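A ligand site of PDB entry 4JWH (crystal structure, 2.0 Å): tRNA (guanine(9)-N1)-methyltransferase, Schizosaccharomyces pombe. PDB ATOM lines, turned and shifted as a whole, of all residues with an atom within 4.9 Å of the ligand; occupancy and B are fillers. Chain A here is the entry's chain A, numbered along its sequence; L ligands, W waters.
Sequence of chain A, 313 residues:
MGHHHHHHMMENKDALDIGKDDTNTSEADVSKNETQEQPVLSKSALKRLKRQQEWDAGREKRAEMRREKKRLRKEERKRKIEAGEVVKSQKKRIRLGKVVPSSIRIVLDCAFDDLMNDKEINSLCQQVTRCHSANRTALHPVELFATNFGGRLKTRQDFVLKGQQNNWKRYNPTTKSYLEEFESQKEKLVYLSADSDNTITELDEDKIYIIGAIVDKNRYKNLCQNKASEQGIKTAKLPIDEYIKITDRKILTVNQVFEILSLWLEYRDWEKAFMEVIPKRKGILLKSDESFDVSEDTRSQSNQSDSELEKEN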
ATOM      1  N   TYR A 191      -4.472  -9.677 -26.458  1.00  0.00           N
ATOM      2  CA  TYR A 191      -5.702  -9.632 -25.688  1.00  0.00           C
ATOM      3  C   TYR A 191      -5.572  -8.546 -24.609  1.00  0.00           C
ATOM      4  O   TYR A 191      -4.738  -8.638 -23.705  1.00  0.00           O
ATOM      5  CB  TYR A 191      -5.988 -10.993 -25.054  1.00  0.00           C
ATOM      6  CG  TYR A 191      -7.471 -11.300 -24.844  1.00  0.00           C
ATOM      7  CD1 TYR A 191      -8.013 -12.485 -25.317  1.00  0.00           C
ATOM      8  CD2 TYR A 191      -8.305 -10.430 -24.121  1.00  0.00           C
ATOM      9  CE1 TYR A 191      -9.354 -12.800 -25.135  1.00  0.00           C
ATOM     10  CE2 TYR A 191      -9.672 -10.720 -23.937  1.00  0.00           C
ATOM     11  CZ  TYR A 191     -10.172 -11.919 -24.470  1.00  0.00           C
ATOM     12  OH  TYR A 191     -11.470 -12.286 -24.315  1.00  0.00           O
ATOM     13  N   LEU A 192      -6.397  -7.520 -24.725  1.00  0.00           N
ATOM     14  CA  LEU A 192      -6.446  -6.437 -23.727  1.00  0.00           C
ATOM     15  C   LEU A 192      -7.077  -6.946 -22.417  1.00  0.00           C
ATOM     16  O   LEU A 192      -8.176  -7.507 -22.426  1.00  0.00           O
ATOM     17  CB  LEU A 192      -7.227  -5.265 -24.300  1.00  0.00           C
ATOM     18  CG  LEU A 192      -6.494  -4.609 -25.508  1.00  0.00           C
ATOM     19  CD1 LEU A 192      -7.333  -3.564 -26.165  1.00  0.00           C
ATOM     20  CD2 LEU A 192      -5.155  -3.978 -25.060  1.00  0.00           C
ATOM     21  N   SER A 193      -6.369  -6.763 -21.303  1.00  0.00           N
ATOM     22  CA  SER A 193      -6.879  -7.160 -19.979  1.00  0.00           C
ATOM     23  C   SER A 193      -6.368  -6.214 -18.881  1.00  0.00           C
ATOM     24  O   SER A 193      -5.175  -5.905 -18.833  1.00  0.00           O
ATOM     25  CB  SER A 193      -6.483  -8.635 -19.670  1.00  0.00           C
ATOM     26  OG  SER A 193      -6.670  -8.973 -18.292  1.00  0.00           O
ATOM     27  N   ALA A 194      -7.257  -5.763 -18.004  1.00  0.00           N
ATOM     28  CA  ALA A 194      -6.824  -4.949 -16.859  1.00  0.00           C
ATOM     29  C   ALA A 194      -5.824  -5.695 -15.940  1.00  0.00           C
ATOM     30  O   ALA A 194      -5.076  -5.073 -15.194  1.00  0.00           O
ATOM     31  CB  ALA A 194      -8.022  -4.444 -16.084  1.00  0.00           C
ATOM     32  N   ASP A 195      -5.835  -7.017 -16.009  1.00  0.00           N
ATOM     33  CA  ASP A 195      -5.030  -7.902 -15.158  1.00  0.00           C
ATOM     34  C   ASP A 195      -3.634  -8.239 -15.674  1.00  0.00           C
ATOM     35  O   ASP A 195      -2.849  -8.898 -14.984  1.00  0.00           O
ATOM     36  CB  ASP A 195      -5.830  -9.191 -14.878  1.00  0.00           C
ATOM     37  CG  ASP A 195      -7.227  -8.884 -14.276  1.00  0.00           C
ATOM     38  OD1 ASP A 195      -7.301  -8.067 -13.324  1.00  0.00           O
ATOM     39  OD2 ASP A 195      -8.265  -9.436 -14.749  1.00  0.00           O
ATOM     40  N   ILE A 210      -7.721  -7.576 -29.013  1.00  0.00           N
ATOM     41  CA  ILE A 210      -8.940  -8.257 -28.587  1.00  0.00           C
ATOM     42  C   ILE A 210      -9.517  -7.596 -27.348  1.00  0.00           C
ATOM     43  O   ILE A 210      -8.787  -7.340 -26.392  1.00  0.00           O
ATOM     44  CB  ILE A 210      -8.710  -9.753 -28.289  1.00  0.00           C
ATOM     45  CG1 ILE A 210      -8.038 -10.447 -29.494  1.00  0.00           C
ATOM     46  CG2 ILE A 210     -10.031 -10.476 -27.964  1.00  0.00           C
ATOM     47  CD1 ILE A 210      -7.263 -11.707 -29.083  1.00  0.00           C
ATOM     48  N   ILE A 211     -10.823  -7.333 -27.362  1.00  0.00           N
ATOM     49  CA  ILE A 211     -11.584  -6.911 -26.170  1.00  0.00           C
ATOM     50  C   ILE A 211     -12.501  -8.066 -25.751  1.00  0.00           C
ATOM     51  O   ILE A 211     -13.232  -8.627 -26.596  1.00  0.00           O
ATOM     52  CB  ILE A 211     -12.425  -5.638 -26.452  1.00  0.00           C
ATOM     53  CG1 ILE A 211     -11.516  -4.528 -27.035  1.00  0.00           C
ATOM     54  CG2 ILE A 211     -13.168  -5.198 -25.172  1.00  0.00           C
ATOM     55  CD1 ILE A 211     -12.260  -3.321 -27.608  1.00  0.00           C
ATOM     56  N   GLY A 212     -12.464  -8.441 -24.470  1.00  0.00           N
ATOM     57  CA  GLY A 212     -13.463  -9.390 -23.935  1.00  0.00           C
ATOM     58  C   GLY A 212     -14.893  -8.869 -23.989  1.00  0.00           C
ATOM     59  O   GLY A 212     -15.212  -7.839 -23.387  1.00  0.00           O
ATOM     60  N   ILE A 214     -17.838  -8.992 -22.490  1.00  0.00           N
ATOM     61  CA  ILE A 214     -18.503  -9.443 -21.275  1.00  0.00           C
ATOM     62  C   ILE A 214     -18.797  -8.267 -20.322  1.00  0.00           C
ATOM     63  O   ILE A 214     -17.992  -7.361 -20.147  1.00  0.00           O
ATOM     64  CB  ILE A 214     -17.680 -10.552 -20.550  1.00  0.00           C
ATOM     65  CG1 ILE A 214     -18.483 -11.151 -19.358  1.00  0.00           C
ATOM     66  CG2 ILE A 214     -16.271 -10.056 -20.154  1.00  0.00           C
ATOM     67  CD1 ILE A 214     -17.844 -12.342 -18.690  1.00  0.00           C
ATOM     68  N   ASP A 216     -19.525  -8.034 -16.591  1.00  0.00           N
ATOM     69  CA  ASP A 216     -19.480  -8.834 -15.367  1.00  0.00           C
ATOM     70  C   ASP A 216     -19.245  -8.003 -14.105  1.00  0.00           C
ATOM     71  O   ASP A 216     -19.328  -8.536 -13.002  1.00  0.00           O
ATOM     72  CB  ASP A 216     -18.444  -9.981 -15.563  1.00  0.00           C
ATOM     73  CG  ASP A 216     -17.009  -9.511 -15.488  1.00  0.00           C
ATOM     74  OD1 ASP A 216     -16.728  -8.383 -15.914  1.00  0.00           O
ATOM     75  OD2 ASP A 216     -16.139 -10.273 -15.005  1.00  0.00           O
ATOM     76  N   ASN A 218     -16.441  -6.969 -13.439  1.00  0.00           N
ATOM     77  CA  ASN A 218     -15.222  -7.635 -13.045  1.00  0.00           C
ATOM     78  C   ASN A 218     -15.323  -8.710 -11.923  1.00  0.00           C
ATOM     79  O   ASN A 218     -14.337  -8.994 -11.248  1.00  0.00           O
ATOM     80  CB  ASN A 218     -14.112  -6.625 -12.727  1.00  0.00           C
ATOM     81  CG  ASN A 218     -12.734  -7.225 -12.888  1.00  0.00           C
ATOM     82  OD1 ASN A 218     -12.476  -7.979 -13.840  1.00  0.00           O
ATOM     83  ND2 ASN A 218     -11.838  -6.908 -11.954  1.00  0.00           N
ATOM     84  N   TYR A 220     -15.489 -11.717 -12.603  1.00  0.00           N
ATOM     85  CA  TYR A 220     -14.602 -12.733 -13.135  1.00  0.00           C
ATOM     86  C   TYR A 220     -13.161 -12.254 -13.293  1.00  0.00           C
ATOM     87  O   TYR A 220     -12.686 -12.086 -14.402  1.00  0.00           O
ATOM     88  CB  TYR A 220     -15.126 -13.318 -14.447  1.00  0.00           C
ATOM     89  CG  TYR A 220     -16.530 -13.835 -14.334  1.00  0.00           C
ATOM     90  CD1 TYR A 220     -16.819 -14.939 -13.544  1.00  0.00           C
ATOM     91  CD2 TYR A 220     -17.556 -13.218 -15.026  1.00  0.00           C
ATOM     92  CE1 TYR A 220     -18.145 -15.426 -13.438  1.00  0.00           C
ATOM     93  CE2 TYR A 220     -18.876 -13.667 -14.911  1.00  0.00           C
ATOM     94  CZ  TYR A 220     -19.156 -14.773 -14.121  1.00  0.00           C
ATOM     95  OH  TYR A 220     -20.461 -15.213 -14.054  1.00  0.00           O
ATOM     96  N   LYS A 221     -12.475 -12.071 -12.162  1.00  0.00           N
ATOM     97  CA  LYS A 221     -11.101 -11.565 -12.157  1.00  0.00           C
ATOM     98  C   LYS A 221     -10.243 -12.537 -12.909  1.00  0.00           C
ATOM     99  O   LYS A 221     -10.425 -13.726 -12.793  1.00  0.00           O
ATOM    100  CB  LYS A 221     -10.556 -11.439 -10.712  1.00  0.00           C
ATOM    101  CG  LYS A 221     -11.431 -10.655  -9.755  1.00  0.00           C
ATOM    102  CD  LYS A 221     -10.747 -10.563  -8.355  1.00  0.00           C
ATOM    103  CE  LYS A 221     -11.319  -9.435  -7.491  1.00  0.00           C
ATOM    104  NZ  LYS A 221     -10.524  -9.221  -6.208  1.00  0.00           N
ATOM    105  N   ASN A 222      -9.297 -12.022 -13.694  1.00  0.00           N
ATOM    106  CA  ASN A 222      -8.366 -12.864 -14.432  1.00  0.00           C
ATOM    107  C   ASN A 222      -8.953 -13.678 -15.551  1.00  0.00           C
ATOM    108  O   ASN A 222      -8.237 -14.436 -16.181  1.00  0.00           O
ATOM    109  CB  ASN A 222      -7.593 -13.793 -13.501  1.00  0.00           C
ATOM    110  CG  ASN A 222      -6.386 -13.122 -12.945  1.00  0.00           C
ATOM    111  OD1 ASN A 222      -5.361 -13.030 -13.615  1.00  0.00           O
ATOM    112  ND2 ASN A 222      -6.519 -12.595 -11.721  1.00  0.00           N
ATOM    113  N   LEU A 223     -10.242 -13.519 -15.810  1.00  0.00           N
ATOM    114  CA  LEU A 223     -10.879 -14.349 -16.825  1.00  0.00           C
ATOM    115  C   LEU A 223     -10.143 -14.225 -18.162  1.00  0.00           C
ATOM    116  O   LEU A 223      -9.638 -15.229 -18.741  1.00  0.00           O
ATOM    117  CB  LEU A 223     -12.357 -13.955 -16.972  1.00  0.00           C
ATOM    118  CG  LEU A 223     -13.203 -14.615 -18.074  1.00  0.00           C
ATOM    119  CD1 LEU A 223     -13.699 -15.983 -17.668  1.00  0.00           C
ATOM    120  CD2 LEU A 223     -14.371 -13.709 -18.423  1.00  0.00           C
ATOM    121  N   CYS A 224     -10.075 -13.011 -18.674  1.00  0.00           N
ATOM    122  CA  CYS A 224      -9.490 -12.820 -20.013  1.00  0.00           C
ATOM    123  C   CYS A 224      -7.998 -13.065 -19.988  1.00  0.00           C
ATOM    124  O   CYS A 224      -7.433 -13.683 -20.901  1.00  0.00           O
ATOM    125  CB  CYS A 224      -9.890 -11.467 -20.614  1.00  0.00           C
ATOM    126  SG  CYS A 224     -11.691 -11.452 -20.913  1.00  0.00           S
ATOM    127  N   GLN A 225      -7.363 -12.615 -18.898  1.00  0.00           N
ATOM    128  CA  GLN A 225      -5.943 -12.876 -18.750  1.00  0.00           C
ATOM    129  C   GLN A 225      -5.692 -14.384 -18.832  1.00  0.00           C
ATOM    130  O   GLN A 225      -4.742 -14.813 -19.483  1.00  0.00           O
ATOM    131  CB  GLN A 225      -5.393 -12.261 -17.450  1.00  0.00           C
ATOM    132  CG  GLN A 225      -3.883 -12.544 -17.174  1.00  0.00           C
ATOM    133  CD  GLN A 225      -2.925 -11.862 -18.159  1.00  0.00           C
ATOM    134  OE1 GLN A 225      -3.207 -10.792 -18.694  1.00  0.00           O
ATOM    135  NE2 GLN A 225      -1.771 -12.481 -18.388  1.00  0.00           N
ATOM    136  N   ALA A 236      -2.094  -7.159 -22.450  1.00  0.00           N
ATOM    137  CA  ALA A 236      -1.654  -5.806 -22.147  1.00  0.00           C
ATOM    138  C   ALA A 236      -2.808  -5.055 -21.531  1.00  0.00           C
ATOM    139  O   ALA A 236      -3.973  -5.181 -22.001  1.00  0.00           O
ATOM    140  CB  ALA A 236      -1.192  -5.092 -23.410  1.00  0.00           C
ATOM    141  N   LYS A 237      -2.529  -4.277 -20.481  1.00  0.00           N
ATOM    142  CA  LYS A 237      -3.517  -3.363 -19.928  1.00  0.00           C
ATOM    143  C   LYS A 237      -3.311  -1.953 -20.447  1.00  0.00           C
ATOM    144  O   LYS A 237      -2.212  -1.575 -20.824  1.00  0.00           O
ATOM    145  CB  LYS A 237      -3.447  -3.360 -18.412  1.00  0.00           C
ATOM    146  CG  LYS A 237      -2.178  -2.741 -17.861  1.00  0.00           C
ATOM    147  CD  LYS A 237      -2.114  -2.955 -16.391  1.00  0.00           C
ATOM    148  CE  LYS A 237      -0.664  -2.867 -15.870  1.00  0.00           C
ATOM    149  NZ  LYS A 237      -0.821  -2.214 -14.540  1.00  0.00           N
ATOM    150  N   LEU A 238      -4.393  -1.180 -20.446  1.00  0.00           N
ATOM    151  CA  LEU A 238      -4.360   0.213 -20.852  1.00  0.00           C
ATOM    152  C   LEU A 238      -3.452   1.007 -19.880  1.00  0.00           C
ATOM    153  O   LEU A 238      -3.413   0.679 -18.672  1.00  0.00           O
ATOM    154  CB  LEU A 238      -5.769   0.811 -20.848  1.00  0.00           C
ATOM    155  CG  LEU A 238      -6.696   0.369 -21.985  1.00  0.00           C
ATOM    156  CD1 LEU A 238      -8.077   0.954 -21.806  1.00  0.00           C
ATOM    157  CD2 LEU A 238      -6.121   0.781 -23.330  1.00  0.00           C
ATOM    158  N   ILE A 240      -3.567   3.288 -17.922  1.00  0.00           N
ATOM    159  CA  ILE A 240      -4.520   4.117 -17.198  1.00  0.00           C
ATOM    160  C   ILE A 240      -3.825   4.809 -16.032  1.00  0.00           C
ATOM    161  O   ILE A 240      -3.873   6.042 -15.936  1.00  0.00           O
ATOM    162  CB  ILE A 240      -5.729   3.280 -16.732  1.00  0.00           C
ATOM    163  CG1 ILE A 240      -6.718   3.108 -17.871  1.00  0.00           C
ATOM    164  CG2 ILE A 240      -6.425   3.936 -15.568  1.00  0.00           C
ATOM    165  CD1 ILE A 240      -7.980   2.401 -17.475  1.00  0.00           C
ATOM    166  N   LYS A 250     -10.769   1.418 -12.938  1.00  0.00           N
ATOM    167  CA  LYS A 250      -9.684   0.557 -13.429  1.00  0.00           C
ATOM    168  C   LYS A 250     -10.170  -0.378 -14.553  1.00  0.00           C
ATOM    169  O   LYS A 250      -9.522  -0.531 -15.608  1.00  0.00           O
ATOM    170  CB  LYS A 250      -9.087  -0.250 -12.265  1.00  0.00           C
ATOM    171  N   ILE A 251     -11.318  -1.023 -14.338  1.00  0.00           N
ATOM    172  CA  ILE A 251     -11.866  -1.918 -15.357  1.00  0.00           C
ATOM    173  C   ILE A 251     -12.996  -1.219 -16.105  1.00  0.00           C
ATOM    174  O   ILE A 251     -14.059  -0.884 -15.556  1.00  0.00           O
ATOM    175  CB  ILE A 251     -12.217  -3.327 -14.781  1.00  0.00           C
ATOM    176  CG1 ILE A 251     -10.960  -4.026 -14.267  1.00  0.00           C
ATOM    177  CG2 ILE A 251     -12.792  -4.225 -15.865  1.00  0.00           C
ATOM    178  CD1 ILE A 251     -10.378  -3.506 -12.943  1.00  0.00           C
ATOM    179  N   LEU A 252     -12.749  -0.965 -17.382  1.00  0.00           N
ATOM    180  CA  LEU A 252     -13.688  -0.175 -18.173  1.00  0.00           C
ATOM    181  C   LEU A 252     -14.654  -1.102 -18.922  1.00  0.00           C
ATOM    182  O   LEU A 252     -14.422  -2.312 -18.975  1.00  0.00           O
ATOM    183  CB  LEU A 252     -12.915   0.730 -19.130  1.00  0.00           C
ATOM    184  CG  LEU A 252     -11.857   1.664 -18.525  1.00  0.00           C
ATOM    185  CD1 LEU A 252     -11.093   2.361 -19.618  1.00  0.00           C
ATOM    186  CD2 LEU A 252     -12.477   2.667 -17.579  1.00  0.00           C
ATOM    187  N   THR A 253     -15.706  -0.526 -19.503  1.00  0.00           N
ATOM    188  CA  THR A 253     -16.670  -1.323 -20.235  1.00  0.00           C
ATOM    189  C   THR A 253     -16.100  -1.634 -21.638  1.00  0.00           C
ATOM    190  O   THR A 253     -15.122  -0.992 -22.085  1.00  0.00           O
ATOM    191  CB  THR A 253     -18.024  -0.592 -20.402  1.00  0.00           C
ATOM    192  OG1 THR A 253     -17.848   0.530 -21.282  1.00  0.00           O
ATOM    193  CG2 THR A 253     -18.604  -0.124 -19.040  1.00  0.00           C
ATOM    194  N   VAL A 254     -16.703  -2.606 -22.319  1.00  0.00           N
ATOM    195  CA  VAL A 254     -16.313  -2.946 -23.695  1.00  0.00           C
ATOM    196  C   VAL A 254     -16.246  -1.693 -24.568  1.00  0.00           C
ATOM    197  O   VAL A 254     -15.222  -1.429 -25.212  1.00  0.00           O
ATOM    198  CB  VAL A 254     -17.268  -3.987 -24.313  1.00  0.00           C
ATOM    199  CG1 VAL A 254     -16.950  -4.206 -25.804  1.00  0.00           C
ATOM    200  CG2 VAL A 254     -17.241  -5.312 -23.517  1.00  0.00           C
ATOM    201  N   VAL A 257     -13.426   0.917 -23.677  1.00  0.00           N
ATOM    202  CA  VAL A 257     -12.091   0.491 -24.115  1.00  0.00           C
ATOM    203  C   VAL A 257     -11.990   0.706 -25.620  1.00  0.00           C
ATOM    204  O   VAL A 257     -11.040   1.289 -26.103  1.00  0.00           O
ATOM    205  CB  VAL A 257     -11.886  -1.012 -23.769  1.00  0.00           C
ATOM    206  CG1 VAL A 257     -10.646  -1.549 -24.476  1.00  0.00           C
ATOM    207  CG2 VAL A 257     -11.750  -1.154 -22.257  1.00  0.00           C
HETATM  208  N1  LIG L   1     -13.350  -9.746 -15.594  1.00  0.00           N
HETATM  209  C1  LIG L   1     -13.454  -9.461 -17.023  1.00  0.00           C
HETATM  210  C2  LIG L   1     -14.202  -8.117 -17.137  1.00  0.00           C
HETATM  211  C3  LIG L   1     -13.636  -7.268 -18.199  1.00  0.00           C
HETATM  212  S1  LIG L   1     -14.293  -5.746 -18.759  1.00  0.00           S
HETATM  213  C4  LIG L   1     -12.085  -9.699 -17.634  1.00  0.00           C
HETATM  214  O1  LIG L   1     -11.607  -9.115 -18.564  1.00  0.00           O
HETATM  215  O2  LIG L   1     -11.407 -10.591 -17.218  1.00  0.00           O
HETATM  216  C5  LIG L   1     -14.456  -6.043 -20.468  1.00  0.00           C
HETATM  217  C6  LIG L   1     -13.203  -5.944 -21.339  1.00  0.00           C
HETATM  218  O3  LIG L   1     -12.718  -4.644 -21.433  1.00  0.00           O
HETATM  219  C7  LIG L   1     -11.998  -6.804 -20.946  1.00  0.00           C
HETATM  220  O4  LIG L   1     -12.121  -8.133 -21.367  1.00  0.00           O
HETATM  221  C8  LIG L   1     -10.845  -6.100 -21.569  1.00  0.00           C
HETATM  222  O5  LIG L   1     -10.713  -6.546 -22.879  1.00  0.00           O
HETATM  223  C9  LIG L   1     -11.314  -4.676 -21.505  1.00  0.00           C
HETATM  224  N2  LIG L   1     -10.691  -3.901 -20.422  1.00  0.00           N
HETATM  225  C10 LIG L   1     -11.303  -3.339 -19.412  1.00  0.00           C
HETATM  226  N3  LIG L   1     -10.492  -2.649 -18.645  1.00  0.00           N
HETATM  227  C11 LIG L   1      -9.325  -2.742 -19.195  1.00  0.00           C
HETATM  228  C12 LIG L   1      -7.970  -2.246 -18.897  1.00  0.00           C
HETATM  229  N4  LIG L   1      -7.750  -1.512 -17.841  1.00  0.00           N
HETATM  230  N5  LIG L   1      -7.010  -2.566 -19.719  1.00  0.00           N
HETATM  231  C13 LIG L   1      -7.223  -3.319 -20.789  1.00  0.00           C
HETATM  232  N6  LIG L   1      -8.392  -3.810 -21.109  1.00  0.00           N
HETATM  233  C14 LIG L   1      -9.470  -3.555 -20.373  1.00  0.00           C
HETATM  234  O   HOH W   1     -10.139  -6.753 -17.920  1.00  0.00           O
HETATM  235  O   HOH W   2      -5.268  -0.504 -16.822  1.00  0.00           O
HETATM  236  O   HOH W   3      -8.632 -10.580 -17.115  1.00  0.00           O
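The backbone carbonyl oxygen (O) of Leu 192 lies within hydrogen-bond range of an oxygen (O5) of the ligand, at 2.8 Å. The side-chain carboxylate of Asp 216 is in salt-bridge range of a nitrogen (N1) of the ligand, 2.9 Å away. The backbone carbonyl oxygen (O) of Lys 250 is in hydrogen-bond range of a nitrogen (N4) of the ligand, 3.0 Å away. An oxygen (O5) of the ligand is in hydrogen-bond range of the backbone NH of Gly 212, at 3.0 Å. The backbone NH (N) of Leu 223 lies within hydrogen-bond range of an oxygen (O2) of the ligand, at 3.5 Å. O2 of the ligand is in hydrogen-bond range of N of Cys 224 (3.1 Å). The backbone NH (N) of Leu 252 lies within hydrogen-bond range of a nitrogen (N3) of the ligand, at 3.1 Å. SG of Cys 224 lies within hydrogen-bond range of O1 of the ligand (3.3 Å). N1 of the ligand is in hydrogen-bond range of O of Tyr 220, at 2.7 Å. N of Leu 238 lies within hydrogen-bond range of N5 of the ligand, at 3.0 Å. OD1 of Asn 218 lies within hydrogen-bond range of N1 of the ligand.
N of Asn 218 sits at hydrogen-bond distance from OD1 of Asp 216 (2.9 Å). The backbone NH of Ser 193 is in hydrogen-bond range of the backbone carbonyl oxygen of Ala 236, at 3.0 Å. OH of Tyr 191 is in hydrogen-bond range of SG of Cys 224, 3.5 Å away. N of Tyr 220 lies within hydrogen-bond range of OD2 of Asp 216 (2.9 Å). The backbone NH of Ala 236 lies within hydrogen-bond range of the backbone carbonyl oxygen of Tyr 191 (3.3 Å). The side-chain hydroxyl (OG) of Ser 193 sits close to the backbone NH (N) of Asp 195, 3.1 Å away. O of Ile 210 sits at hydrogen-bond distance from N of Leu 192.
Ser 193 touches the ligand (C to C13, 3.6 Å). Ala 194 touches the ligand. CA of Ile 211 touches O5 of the ligand, at 3.4 Å. Ile 214 touches the ligand. Ala 236 touches the ligand (O to C13, 3.9 Å). Lys 237 touches the ligand. CD1 of Ile 240 touches N4 of the ligand, 3.9 Å away. CG2 of Ile 251 touches S1 of the ligand (3.6 Å). Val 257 touches the ligand. Hydrophobic or aromatic side chains within 4 Å of the ligand: Leu 192, Ala 194, Ile 211, Leu 223, Leu 238, Ile 240, Ile 251 and Val 257. The nearest printed residue that does not touch the ligand is Ile 210 (4.1 Å).
Water W3 lies within hydrogen-bond range of the side-chain carboxylate (OD2) of Asp 195, an oxygen (O2) of the ligand, the side-chain hydroxyl (OG) of Ser 193, the backbone NH (N) of Gln 225 and the backbone NH (N) of Cys 224. Water W1 bridges O1 of the ligand and N of Ala 194. Water W2 lies within hydrogen-bond range of a nitrogen (N4) of the ligand and the backbone carbonyl oxygen of Leu 238.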
